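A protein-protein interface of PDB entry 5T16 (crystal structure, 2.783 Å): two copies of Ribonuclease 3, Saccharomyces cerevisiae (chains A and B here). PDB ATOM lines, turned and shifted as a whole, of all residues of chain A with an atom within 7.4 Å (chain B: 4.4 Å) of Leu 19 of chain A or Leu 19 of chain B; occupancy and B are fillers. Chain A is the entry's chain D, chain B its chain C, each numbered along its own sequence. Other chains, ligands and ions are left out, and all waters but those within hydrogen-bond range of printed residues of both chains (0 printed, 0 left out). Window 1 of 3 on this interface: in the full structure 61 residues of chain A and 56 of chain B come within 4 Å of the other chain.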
ATOM      1  N   LEU A  12     -25.568  23.919  -7.248  1.00  0.00           N
ATOM      2  CA  LEU A  12     -24.978  22.938  -8.131  1.00  0.00           C
ATOM      3  C   LEU A  12     -24.151  23.574  -9.219  1.00  0.00           C
ATOM      4  O   LEU A  12     -23.005  23.191  -9.438  1.00  0.00           O
ATOM      5  CB  LEU A  12     -26.050  22.071  -8.774  1.00  0.00           C
ATOM      6  CG  LEU A  12     -26.395  20.795  -8.020  1.00  0.00           C
ATOM      7  CD1 LEU A  12     -27.604  20.123  -8.665  1.00  0.00           C
ATOM      8  CD2 LEU A  12     -25.174  19.874  -8.019  1.00  0.00           C
ATOM      9  N   GLU A  13     -24.749  24.562  -9.877  1.00  0.00           N
ATOM     10  CA  GLU A  13     -24.128  25.280 -10.964  1.00  0.00           C
ATOM     11  C   GLU A  13     -22.840  25.899 -10.490  1.00  0.00           C
ATOM     12  O   GLU A  13     -21.811  25.837 -11.167  1.00  0.00           O
ATOM     13  CB  GLU A  13     -25.078  26.352 -11.494  1.00  0.00           C
ATOM     14  CG  GLU A  13     -26.188  25.798 -12.381  1.00  0.00           C
ATOM     15  CD  GLU A  13     -27.025  26.873 -13.036  1.00  0.00           C
ATOM     16  OE1 GLU A  13     -27.547  27.752 -12.320  1.00  0.00           O
ATOM     17  OE2 GLU A  13     -27.152  26.839 -14.278  1.00  0.00           O
ATOM     18  N   HIS A  14     -22.906  26.520  -9.324  1.00  0.00           N
ATOM     19  CA  HIS A  14     -21.748  27.182  -8.761  1.00  0.00           C
ATOM     20  C   HIS A  14     -20.683  26.160  -8.383  1.00  0.00           C
ATOM     21  O   HIS A  14     -19.505  26.389  -8.604  1.00  0.00           O
ATOM     22  CB  HIS A  14     -22.157  28.036  -7.566  1.00  0.00           C
ATOM     23  CG  HIS A  14     -21.076  28.945  -7.070  1.00  0.00           C
ATOM     24  ND1 HIS A  14     -21.268  29.831  -6.032  1.00  0.00           N
ATOM     25  CD2 HIS A  14     -19.803  29.136  -7.495  1.00  0.00           C
ATOM     26  CE1 HIS A  14     -20.161  30.522  -5.832  1.00  0.00           C
ATOM     27  NE2 HIS A  14     -19.254  30.113  -6.700  1.00  0.00           N
ATOM     28  N   ALA A  15     -21.100  25.030  -7.818  1.00  0.00           N
ATOM     29  CA  ALA A  15     -20.152  24.008  -7.363  1.00  0.00           C
ATOM     30  C   ALA A  15     -19.380  23.469  -8.538  1.00  0.00           C
ATOM     31  O   ALA A  15     -18.185  23.289  -8.451  1.00  0.00           O
ATOM     32  CB  ALA A  15     -20.865  22.873  -6.626  1.00  0.00           C
ATOM     33  N   VAL A  16     -20.082  23.206  -9.630  1.00  0.00           N
ATOM     34  CA  VAL A  16     -19.479  22.737 -10.871  1.00  0.00           C
ATOM     35  C   VAL A  16     -18.448  23.717 -11.431  1.00  0.00           C
ATOM     36  O   VAL A  16     -17.388  23.321 -11.906  1.00  0.00           O
ATOM     37  CB  VAL A  16     -20.559  22.496 -11.936  1.00  0.00           C
ATOM     38  CG1 VAL A  16     -19.937  22.288 -13.282  1.00  0.00           C
ATOM     39  CG2 VAL A  16     -21.428  21.327 -11.558  1.00  0.00           C
ATOM     40  N   THR A  17     -18.783  24.997 -11.410  1.00  0.00           N
ATOM     41  CA  THR A  17     -17.851  26.016 -11.856  1.00  0.00           C
ATOM     42  C   THR A  17     -16.570  25.965 -10.998  1.00  0.00           C
ATOM     43  O   THR A  17     -15.466  25.974 -11.534  1.00  0.00           O
ATOM     44  CB  THR A  17     -18.492  27.418 -11.822  1.00  0.00           C
ATOM     45  OG1 THR A  17     -19.503  27.499 -12.825  1.00  0.00           O
ATOM     46  CG2 THR A  17     -17.473  28.496 -12.081  1.00  0.00           C
ATOM     47  N   LYS A  18     -16.700  25.941  -9.675  1.00  0.00           N
ATOM     48  CA  LYS A  18     -15.502  25.885  -8.847  1.00  0.00           C
ATOM     49  C   LYS A  18     -14.735  24.609  -9.139  1.00  0.00           C
ATOM     50  O   LYS A  18     -13.507  24.614  -9.225  1.00  0.00           O
ATOM     51  CB  LYS A  18     -15.828  25.954  -7.352  1.00  0.00           C
ATOM     52  CG  LYS A  18     -16.260  27.325  -6.842  1.00  0.00           C
ATOM     53  CD  LYS A  18     -16.083  27.469  -5.315  1.00  0.00           C
ATOM     54  CE  LYS A  18     -16.461  28.882  -4.849  1.00  0.00           C
ATOM     55  NZ  LYS A  18     -16.243  29.118  -3.387  1.00  0.00           N
ATOM     56  N   LEU A  19     -15.476  23.528  -9.354  1.00  0.00           N
ATOM     57  CA  LEU A  19     -14.870  22.238  -9.589  1.00  0.00           C
ATOM     58  C   LEU A  19     -13.895  22.346 -10.750  1.00  0.00           C
ATOM     59  O   LEU A  19     -12.737  21.957 -10.653  1.00  0.00           O
ATOM     60  CB  LEU A  19     -15.927  21.181  -9.888  1.00  0.00           C
ATOM     61  CG  LEU A  19     -15.263  19.817 -10.108  1.00  0.00           C
ATOM     62  CD1 LEU A  19     -14.745  19.299  -8.783  1.00  0.00           C
ATOM     63  CD2 LEU A  19     -16.142  18.779 -10.818  1.00  0.00           C
ATOM     64  N   VAL A  20     -14.371  22.881 -11.858  1.00  0.00           N
ATOM     65  CA  VAL A  20     -13.554  22.991 -13.046  1.00  0.00           C
ATOM     66  C   VAL A  20     -12.397  23.983 -12.863  1.00  0.00           C
ATOM     67  O   VAL A  20     -11.248  23.661 -13.143  1.00  0.00           O
ATOM     68  CB  VAL A  20     -14.423  23.415 -14.211  1.00  0.00           C
ATOM     69  CG1 VAL A  20     -13.572  23.672 -15.400  1.00  0.00           C
ATOM     70  CG2 VAL A  20     -15.453  22.331 -14.490  1.00  0.00           C
ATOM     71  N   GLU A  21     -12.710  25.159 -12.319  1.00  0.00           N
ATOM     72  CA  GLU A  21     -11.729  26.214 -12.112  1.00  0.00           C
ATOM     73  C   GLU A  21     -10.592  25.710 -11.251  1.00  0.00           C
ATOM     74  O   GLU A  21      -9.427  26.015 -11.470  1.00  0.00           O
ATOM     75  CB  GLU A  21     -12.377  27.422 -11.438  1.00  0.00           C
ATOM     76  CG  GLU A  21     -12.634  28.607 -12.351  1.00  0.00           C
ATOM     77  CD  GLU A  21     -13.833  29.471 -11.895  1.00  0.00           C
ATOM     78  OE1 GLU A  21     -14.169  29.423 -10.671  1.00  0.00           O
ATOM     79  OE2 GLU A  21     -14.425  30.190 -12.757  1.00  0.00           O
ATOM     80  N   SER A  22     -10.947  24.903 -10.275  1.00  0.00           N
ATOM     81  CA  SER A  22      -9.987  24.389  -9.333  1.00  0.00           C
ATOM     82  C   SER A  22      -9.047  23.391  -9.994  1.00  0.00           C
ATOM     83  O   SER A  22      -7.845  23.430  -9.752  1.00  0.00           O
ATOM     84  CB  SER A  22     -10.711  23.764  -8.141  1.00  0.00           C
ATOM     85  OG  SER A  22     -11.299  24.786  -7.358  1.00  0.00           O
ATOM     86  N   TYR A  23      -9.580  22.469 -10.788  1.00  0.00           N
ATOM     87  CA  TYR A  23      -8.693  21.532 -11.460  1.00  0.00           C
ATOM     88  C   TYR A  23      -7.731  22.240 -12.425  1.00  0.00           C
ATOM     89  O   TYR A  23      -6.527  21.965 -12.429  1.00  0.00           O
ATOM     90  CB  TYR A  23      -9.486  20.472 -12.193  1.00  0.00           C
ATOM     91  CG  TYR A  23      -8.587  19.475 -12.865  1.00  0.00           C
ATOM     92  CD1 TYR A  23      -7.733  18.689 -12.117  1.00  0.00           C
ATOM     93  CD2 TYR A  23      -8.623  19.281 -14.235  1.00  0.00           C
ATOM     94  CE1 TYR A  23      -6.908  17.759 -12.721  1.00  0.00           C
ATOM     95  CE2 TYR A  23      -7.810  18.347 -14.844  1.00  0.00           C
ATOM     96  CZ  TYR A  23      -6.956  17.590 -14.080  1.00  0.00           C
ATOM     97  OH  TYR A  23      -6.135  16.661 -14.660  1.00  0.00           O
ATOM     98  N   ASN A  24      -8.263  23.190 -13.193  1.00  0.00           N
ATOM     99  CA  ASN A  24      -7.463  23.992 -14.096  1.00  0.00           C
ATOM    100  C   ASN A  24      -6.321  24.671 -13.367  1.00  0.00           C
ATOM    101  O   ASN A  24      -5.206  24.700 -13.877  1.00  0.00           O
ATOM    102  CB  ASN A  24      -8.326  25.024 -14.813  1.00  0.00           C
ATOM    103  CG  ASN A  24      -9.141  24.413 -15.939  1.00  0.00           C
ATOM    104  OD1 ASN A  24      -8.933  23.257 -16.301  1.00  0.00           O
ATOM    105  ND2 ASN A  24     -10.064  25.184 -16.499  1.00  0.00           N
ATOM    106  N   LYS A  25      -6.597  25.248 -12.203  1.00  0.00           N
ATOM    107  CA  LYS A  25      -5.553  25.922 -11.428  1.00  0.00           C
ATOM    108  C   LYS A  25      -4.482  24.936 -10.974  1.00  0.00           C
ATOM    109  O   LYS A  25      -3.305  25.290 -10.858  1.00  0.00           O
ATOM    110  CB  LYS A  25      -6.125  26.649 -10.209  1.00  0.00           C
ATOM    111  CG  LYS A  25      -5.259  27.795  -9.730  1.00  0.00           C
ATOM    112  CD  LYS A  25      -5.247  28.853 -10.796  1.00  0.00           C
ATOM    113  CE  LYS A  25      -4.447  30.073 -10.406  1.00  0.00           C
ATOM    114  NZ  LYS A  25      -4.409  31.029 -11.556  1.00  0.00           N
ATOM    115  N   ILE A  26      -4.906  23.720 -10.652  1.00  0.00           N
ATOM    116  CA  ILE A  26      -3.978  22.708 -10.151  1.00  0.00           C
ATOM    117  C   ILE A  26      -2.994  22.325 -11.244  1.00  0.00           C
ATOM    118  O   ILE A  26      -1.784  22.334 -11.046  1.00  0.00           O
ATOM    119  CB  ILE A  26      -4.709  21.445  -9.669  1.00  0.00           C
ATOM    120  CG1 ILE A  26      -5.560  21.757  -8.449  1.00  0.00           C
ATOM    121  CG2 ILE A  26      -3.718  20.330  -9.370  1.00  0.00           C
ATOM    122  CD1 ILE A  26      -6.502  20.645  -8.102  1.00  0.00           C
ATOM    123  N   LEU A  61      -1.270  15.702  -3.427  1.00  0.00           N
ATOM    124  CA  LEU A  61      -2.405  15.371  -4.289  1.00  0.00           C
ATOM    125  C   LEU A  61      -2.383  16.189  -5.583  1.00  0.00           C
ATOM    126  O   LEU A  61      -2.676  15.668  -6.669  1.00  0.00           O
ATOM    127  CB  LEU A  61      -3.724  15.589  -3.564  1.00  0.00           C
ATOM    128  CG  LEU A  61      -4.950  15.361  -4.442  1.00  0.00           C
ATOM    129  CD1 LEU A  61      -4.874  14.048  -5.161  1.00  0.00           C
ATOM    130  CD2 LEU A  61      -6.193  15.386  -3.605  1.00  0.00           C
ATOM    131  N   LEU A  65      -1.909  14.635  -9.399  1.00  0.00           N
ATOM    132  CA  LEU A  65      -2.829  14.963 -10.486  1.00  0.00           C
ATOM    133  C   LEU A  65      -2.089  15.551 -11.661  1.00  0.00           C
ATOM    134  O   LEU A  65      -2.386  15.246 -12.803  1.00  0.00           O
ATOM    135  CB  LEU A  65      -3.909  15.928 -10.001  1.00  0.00           C
ATOM    136  CG  LEU A  65      -4.931  15.252  -9.103  1.00  0.00           C
ATOM    137  CD1 LEU A  65      -5.939  16.248  -8.637  1.00  0.00           C
ATOM    138  CD2 LEU A  65      -5.594  14.165  -9.899  1.00  0.00           C
ATOM    139  N   LEU A  77     -10.841  13.485 -16.257  1.00  0.00           N
ATOM    140  CA  LEU A  77     -10.648  14.874 -15.847  1.00  0.00           C
ATOM    141  C   LEU A  77     -10.448  15.789 -17.039  1.00  0.00           C
ATOM    142  O   LEU A  77     -10.845  16.947 -16.991  1.00  0.00           O
ATOM    143  CB  LEU A  77      -9.457  15.025 -14.906  1.00  0.00           C
ATOM    144  CG  LEU A  77      -9.591  14.242 -13.609  1.00  0.00           C
ATOM    145  CD1 LEU A  77      -8.435  14.558 -12.699  1.00  0.00           C
ATOM    146  CD2 LEU A  77     -10.893  14.560 -12.954  1.00  0.00           C
ATOM    147  N   ILE A  80     -13.937  16.613 -18.481  1.00  0.00           N
ATOM    148  CA  ILE A  80     -14.603  17.618 -17.659  1.00  0.00           C
ATOM    149  C   ILE A  80     -14.193  19.050 -17.992  1.00  0.00           C
ATOM    150  O   ILE A  80     -15.047  19.930 -18.121  1.00  0.00           O
ATOM    151  CB  ILE A  80     -14.359  17.347 -16.161  1.00  0.00           C
ATOM    152  CG1 ILE A  80     -15.139  16.102 -15.734  1.00  0.00           C
ATOM    153  CG2 ILE A  80     -14.767  18.538 -15.317  1.00  0.00           C
ATOM    154  CD1 ILE A  80     -14.951  15.722 -14.303  1.00  0.00           C
ATOM    155  N   THR A  81     -12.897  19.299 -18.110  1.00  0.00           N
ATOM    156  CA  THR A  81     -12.429  20.640 -18.466  1.00  0.00           C
ATOM    157  C   THR A  81     -12.818  21.024 -19.892  1.00  0.00           C
ATOM    158  O   THR A  81     -12.882  22.209 -20.221  1.00  0.00           O
ATOM    159  CB  THR A  81     -10.918  20.792 -18.283  1.00  0.00           C
ATOM    160  OG1 THR A  81     -10.223  19.904 -19.168  1.00  0.00           O
ATOM    161  CG2 THR A  81     -10.553  20.455 -16.877  1.00  0.00           C
ATOM    162  N   ALA B  15      -6.897  25.459  -3.973  1.00  0.00           N
ATOM    163  CA  ALA B  15      -7.528  24.808  -5.119  1.00  0.00           C
ATOM    164  C   ALA B  15      -7.895  23.355  -4.832  1.00  0.00           C
ATOM    165  O   ALA B  15      -9.002  22.926  -5.160  1.00  0.00           O
ATOM    166  CB  ALA B  15      -6.622  24.889  -6.332  1.00  0.00           C
ATOM    167  N   VAL B  16      -6.964  22.608  -4.231  1.00  0.00           N
ATOM    168  CA  VAL B  16      -7.213  21.224  -3.832  1.00  0.00           C
ATOM    169  C   VAL B  16      -8.356  21.130  -2.820  1.00  0.00           C
ATOM    170  O   VAL B  16      -9.229  20.265  -2.934  1.00  0.00           O
ATOM    171  CB  VAL B  16      -5.944  20.572  -3.236  1.00  0.00           C
ATOM    172  CG1 VAL B  16      -6.259  19.234  -2.572  1.00  0.00           C
ATOM    173  CG2 VAL B  16      -4.883  20.412  -4.314  1.00  0.00           C
ATOM    174  N   THR B  17      -8.362  22.024  -1.836  1.00  0.00           N
ATOM    175  CA  THR B  17      -9.435  22.035  -0.863  1.00  0.00           C
ATOM    176  C   THR B  17     -10.773  22.228  -1.554  1.00  0.00           C
ATOM    177  O   THR B  17     -11.684  21.436  -1.353  1.00  0.00           O
ATOM    178  CB  THR B  17      -9.239  23.132   0.176  1.00  0.00           C
ATOM    179  OG1 THR B  17      -8.116  22.803   1.006  1.00  0.00           O
ATOM    180  CG2 THR B  17     -10.481  23.272   1.043  1.00  0.00           C
ATOM    181  N   LYS B  18     -10.886  23.263  -2.385  1.00  0.00           N
ATOM    182  CA  LYS B  18     -12.127  23.518  -3.104  1.00  0.00           C
ATOM    183  C   LYS B  18     -12.510  22.409  -4.055  1.00  0.00           C
ATOM    184  O   LYS B  18     -13.686  22.113  -4.247  1.00  0.00           O
ATOM    185  CB  LYS B  18     -12.043  24.828  -3.867  1.00  0.00           C
ATOM    186  CG  LYS B  18     -12.132  26.026  -2.962  1.00  0.00           C
ATOM    187  CD  LYS B  18     -13.226  25.808  -1.942  1.00  0.00           C
ATOM    188  CE  LYS B  18     -13.559  27.073  -1.215  1.00  0.00           C
ATOM    189  NZ  LYS B  18     -14.558  26.752  -0.187  1.00  0.00           N
ATOM    190  N   LEU B  19     -11.509  21.814  -4.677  1.00  0.00           N
ATOM    191  CA  LEU B  19     -11.753  20.735  -5.611  1.00  0.00           C
ATOM    192  C   LEU B  19     -12.550  19.632  -4.950  1.00  0.00           C
ATOM    193  O   LEU B  19     -13.549  19.167  -5.493  1.00  0.00           O
ATOM    194  CB  LEU B  19     -10.453  20.179  -6.139  1.00  0.00           C
ATOM    195  CG  LEU B  19     -10.726  19.021  -7.081  1.00  0.00           C
ATOM    196  CD1 LEU B  19     -11.347  19.562  -8.319  1.00  0.00           C
ATOM    197  CD2 LEU B  19      -9.456  18.279  -7.413  1.00  0.00           C
ATOM    198  N   VAL B  20     -12.080  19.203  -3.782  1.00  0.00           N
ATOM    199  CA  VAL B  20     -12.715  18.129  -3.031  1.00  0.00           C
ATOM    200  C   VAL B  20     -14.092  18.526  -2.506  1.00  0.00           C
ATOM    201  O   VAL B  20     -15.069  17.776  -2.616  1.00  0.00           O
ATOM    202  CB  VAL B  20     -11.847  17.710  -1.842  1.00  0.00           C
ATOM    203  CG1 VAL B  20     -12.621  16.777  -0.918  1.00  0.00           C
ATOM    204  CG2 VAL B  20     -10.558  17.082  -2.329  1.00  0.00           C
ATOM    205  N   GLU B  21     -14.156  19.718  -1.932  1.00  0.00           N
ATOM    206  CA  GLU B  21     -15.389  20.222  -1.379  1.00  0.00           C
ATOM    207  C   GLU B  21     -16.481  20.297  -2.452  1.00  0.00           C
ATOM    208  O   GLU B  21     -17.646  19.984  -2.193  1.00  0.00           O
ATOM    209  CB  GLU B  21     -15.126  21.582  -0.752  1.00  0.00           C
ATOM    210  CG  GLU B  21     -16.362  22.300  -0.295  1.00  0.00           C
ATOM    211  CD  GLU B  21     -16.045  23.619   0.399  1.00  0.00           C
ATOM    212  OE1 GLU B  21     -14.837  23.982   0.491  1.00  0.00           O
ATOM    213  OE2 GLU B  21     -17.014  24.295   0.826  1.00  0.00           O
ATOM    214  N   SER B  22     -16.081  20.668  -3.667  1.00  0.00           N
ATOM    215  CA  SER B  22     -17.001  20.840  -4.788  1.00  0.00           C
ATOM    216  C   SER B  22     -17.583  19.546  -5.338  1.00  0.00           C
ATOM    217  O   SER B  22     -18.797  19.457  -5.539  1.00  0.00           O
ATOM    218  CB  SER B  22     -16.303  21.583  -5.914  1.00  0.00           C
ATOM    219  OG  SER B  22     -16.075  22.930  -5.553  1.00  0.00           O
ATOM    220  N   TYR B  23     -16.723  18.549  -5.583  1.00  0.00           N
ATOM    221  CA  TYR B  23     -17.186  17.254  -6.071  1.00  0.00           C
ATOM    222  C   TYR B  23     -18.170  16.632  -5.069  1.00  0.00           C
ATOM    223  O   TYR B  23     -19.180  16.034  -5.460  1.00  0.00           O
ATOM    224  CB  TYR B  23     -16.025  16.305  -6.319  1.00  0.00           C
ATOM    225  CG  TYR B  23     -16.462  14.948  -6.848  1.00  0.00           C
ATOM    226  CD1 TYR B  23     -17.037  14.822  -8.098  1.00  0.00           C
ATOM    227  CD2 TYR B  23     -16.307  13.789  -6.089  1.00  0.00           C
ATOM    228  CE1 TYR B  23     -17.444  13.584  -8.584  1.00  0.00           C
ATOM    229  CE2 TYR B  23     -16.718  12.547  -6.570  1.00  0.00           C
ATOM    230  CZ  TYR B  23     -17.288  12.456  -7.820  1.00  0.00           C
ATOM    231  OH  TYR B  23     -17.710  11.250  -8.323  1.00  0.00           O
ATOM    232  N   ILE B  26     -21.600  18.202  -5.292  1.00  0.00           N
ATOM    233  CA  ILE B  26     -22.294  17.763  -6.482  1.00  0.00           C
ATOM    234  C   ILE B  26     -22.959  16.416  -6.251  1.00  0.00           C
ATOM    235  O   ILE B  26     -24.156  16.282  -6.472  1.00  0.00           O
ATOM    236  CB  ILE B  26     -21.346  17.668  -7.669  1.00  0.00           C
ATOM    237  CG1 ILE B  26     -20.827  19.060  -8.029  1.00  0.00           C
ATOM    238  CG2 ILE B  26     -22.045  17.003  -8.843  1.00  0.00           C
ATOM    239  CD1 ILE B  26     -19.667  19.053  -8.992  1.00  0.00           C
ATOM    240  N   LEU B  65     -21.842  13.368 -13.892  1.00  0.00           N
ATOM    241  CA  LEU B  65     -20.911  12.946 -12.852  1.00  0.00           C
ATOM    242  C   LEU B  65     -21.592  12.075 -11.823  1.00  0.00           C
ATOM    243  O   LEU B  65     -21.075  11.019 -11.455  1.00  0.00           O
ATOM    244  CB  LEU B  65     -20.283  14.140 -12.140  1.00  0.00           C
ATOM    245  CG  LEU B  65     -19.227  14.959 -12.877  1.00  0.00           C
ATOM    246  CD1 LEU B  65     -18.725  16.101 -12.004  1.00  0.00           C
ATOM    247  CD2 LEU B  65     -18.062  14.093 -13.306  1.00  0.00           C
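Leu 19 of chain A touches five residues of chain B. Printed residues of chain A within 4 Å of Leu 65 of chain B: Leu 19 and Ile 80. Of the printed residues of chain A, Ala 15 of chain B touches Ser 22 and Ile 26. Of the printed residues of chain B, Leu 12 of chain A touches Ile 26 (3.9 Å). The nearest printed residue of chain B that does not touch Leu 12 of chain A is Ser 22 of chain B (6.8 Å).
Ala 15 of chain A touches Ser 22 of chain B, and with the chains exchanged Ser 22 of chain A touches Ala 15 of chain B. Lys 18 of chain A touches Ser 22 of chain B, and with the chains exchanged Ser 22 of chain A touches Lys 18 of chain B. Leu 19 of chain B touches its own counterpart, Leu 19 of chain A. Ile 26 of chain A touches Ala 15 of chain B, but with the chains exchanged Ala 15 of chain A does not touch Ile 26 of chain B (4.1 Å).
Hydrophobic or aromatic side chains of chain B within 4 Å of the printed part of chain A: Ala 15, Val 16, Leu 19, Ile 26 and Leu 65. Hydrophobic or aromatic side chains of chain A within 4 Å of the printed part of chain B: Leu 12, Val 16, Leu 19, Ile 26, Leu 61 and Ile 80. Among the printed residues, no Asp or Glu carboxylate lies within 4 Å of a Lys or Arg side-chain nitrogen of the other chain.
NZ of Lys 18 of chain B is in salt-bridge range of OE1 of Glu 21 of chain B (2.9 Å). The side-chain hydroxyl of Ser 22 of chain B sits at hydrogen-bond distance from the backbone carbonyl oxygen of Lys 18 of chain B. The backbone carbonyl oxygen of Lys 18 of chain A is in hydrogen-bond range of the side-chain hydroxyl of Ser 22 of chain A, 2.9 Å away.
Among the printed residues, pairs that only touch across the chains: Leu 19 of chain A with Leu 19 of chain B (3.4 Å), Lys 18 of chain A with Ser 22 of chain B (3.5 Å), Ser 22 of chain A with Ala 15 of chain B (3.5 Å), Ser 22 of chain A with Lys 18 of chain B (3.6 Å), Ala 15 of chain A with Ser 22 of chain B (3.6 Å), Ile 80 of chain A with Leu 65 of chain B (3.7 Å), Leu 19 of chain A with Tyr 23 of chain B (3.8 Å), Ile 26 of chain A with Leu 19 of chain B (3.8 Å), Val 16 of chain A with Ile 26 of chain B (3.9 Å), Leu 12 of chain A with Ile 26 of chain B (3.9 Å), Leu 19 of chain A with Ser 22 of chain B (3.9 Å), Leu 19 of chain A with Leu 65 of chain B (3.9 Å), Ile 26 of chain A with Ala 15 of chain B (3.9 Å), Leu 19 of chain A with Ile 26 of chain B (3.98 Å) and Leu 61 of chain A with Val 16 of chain B (3.98 Å).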
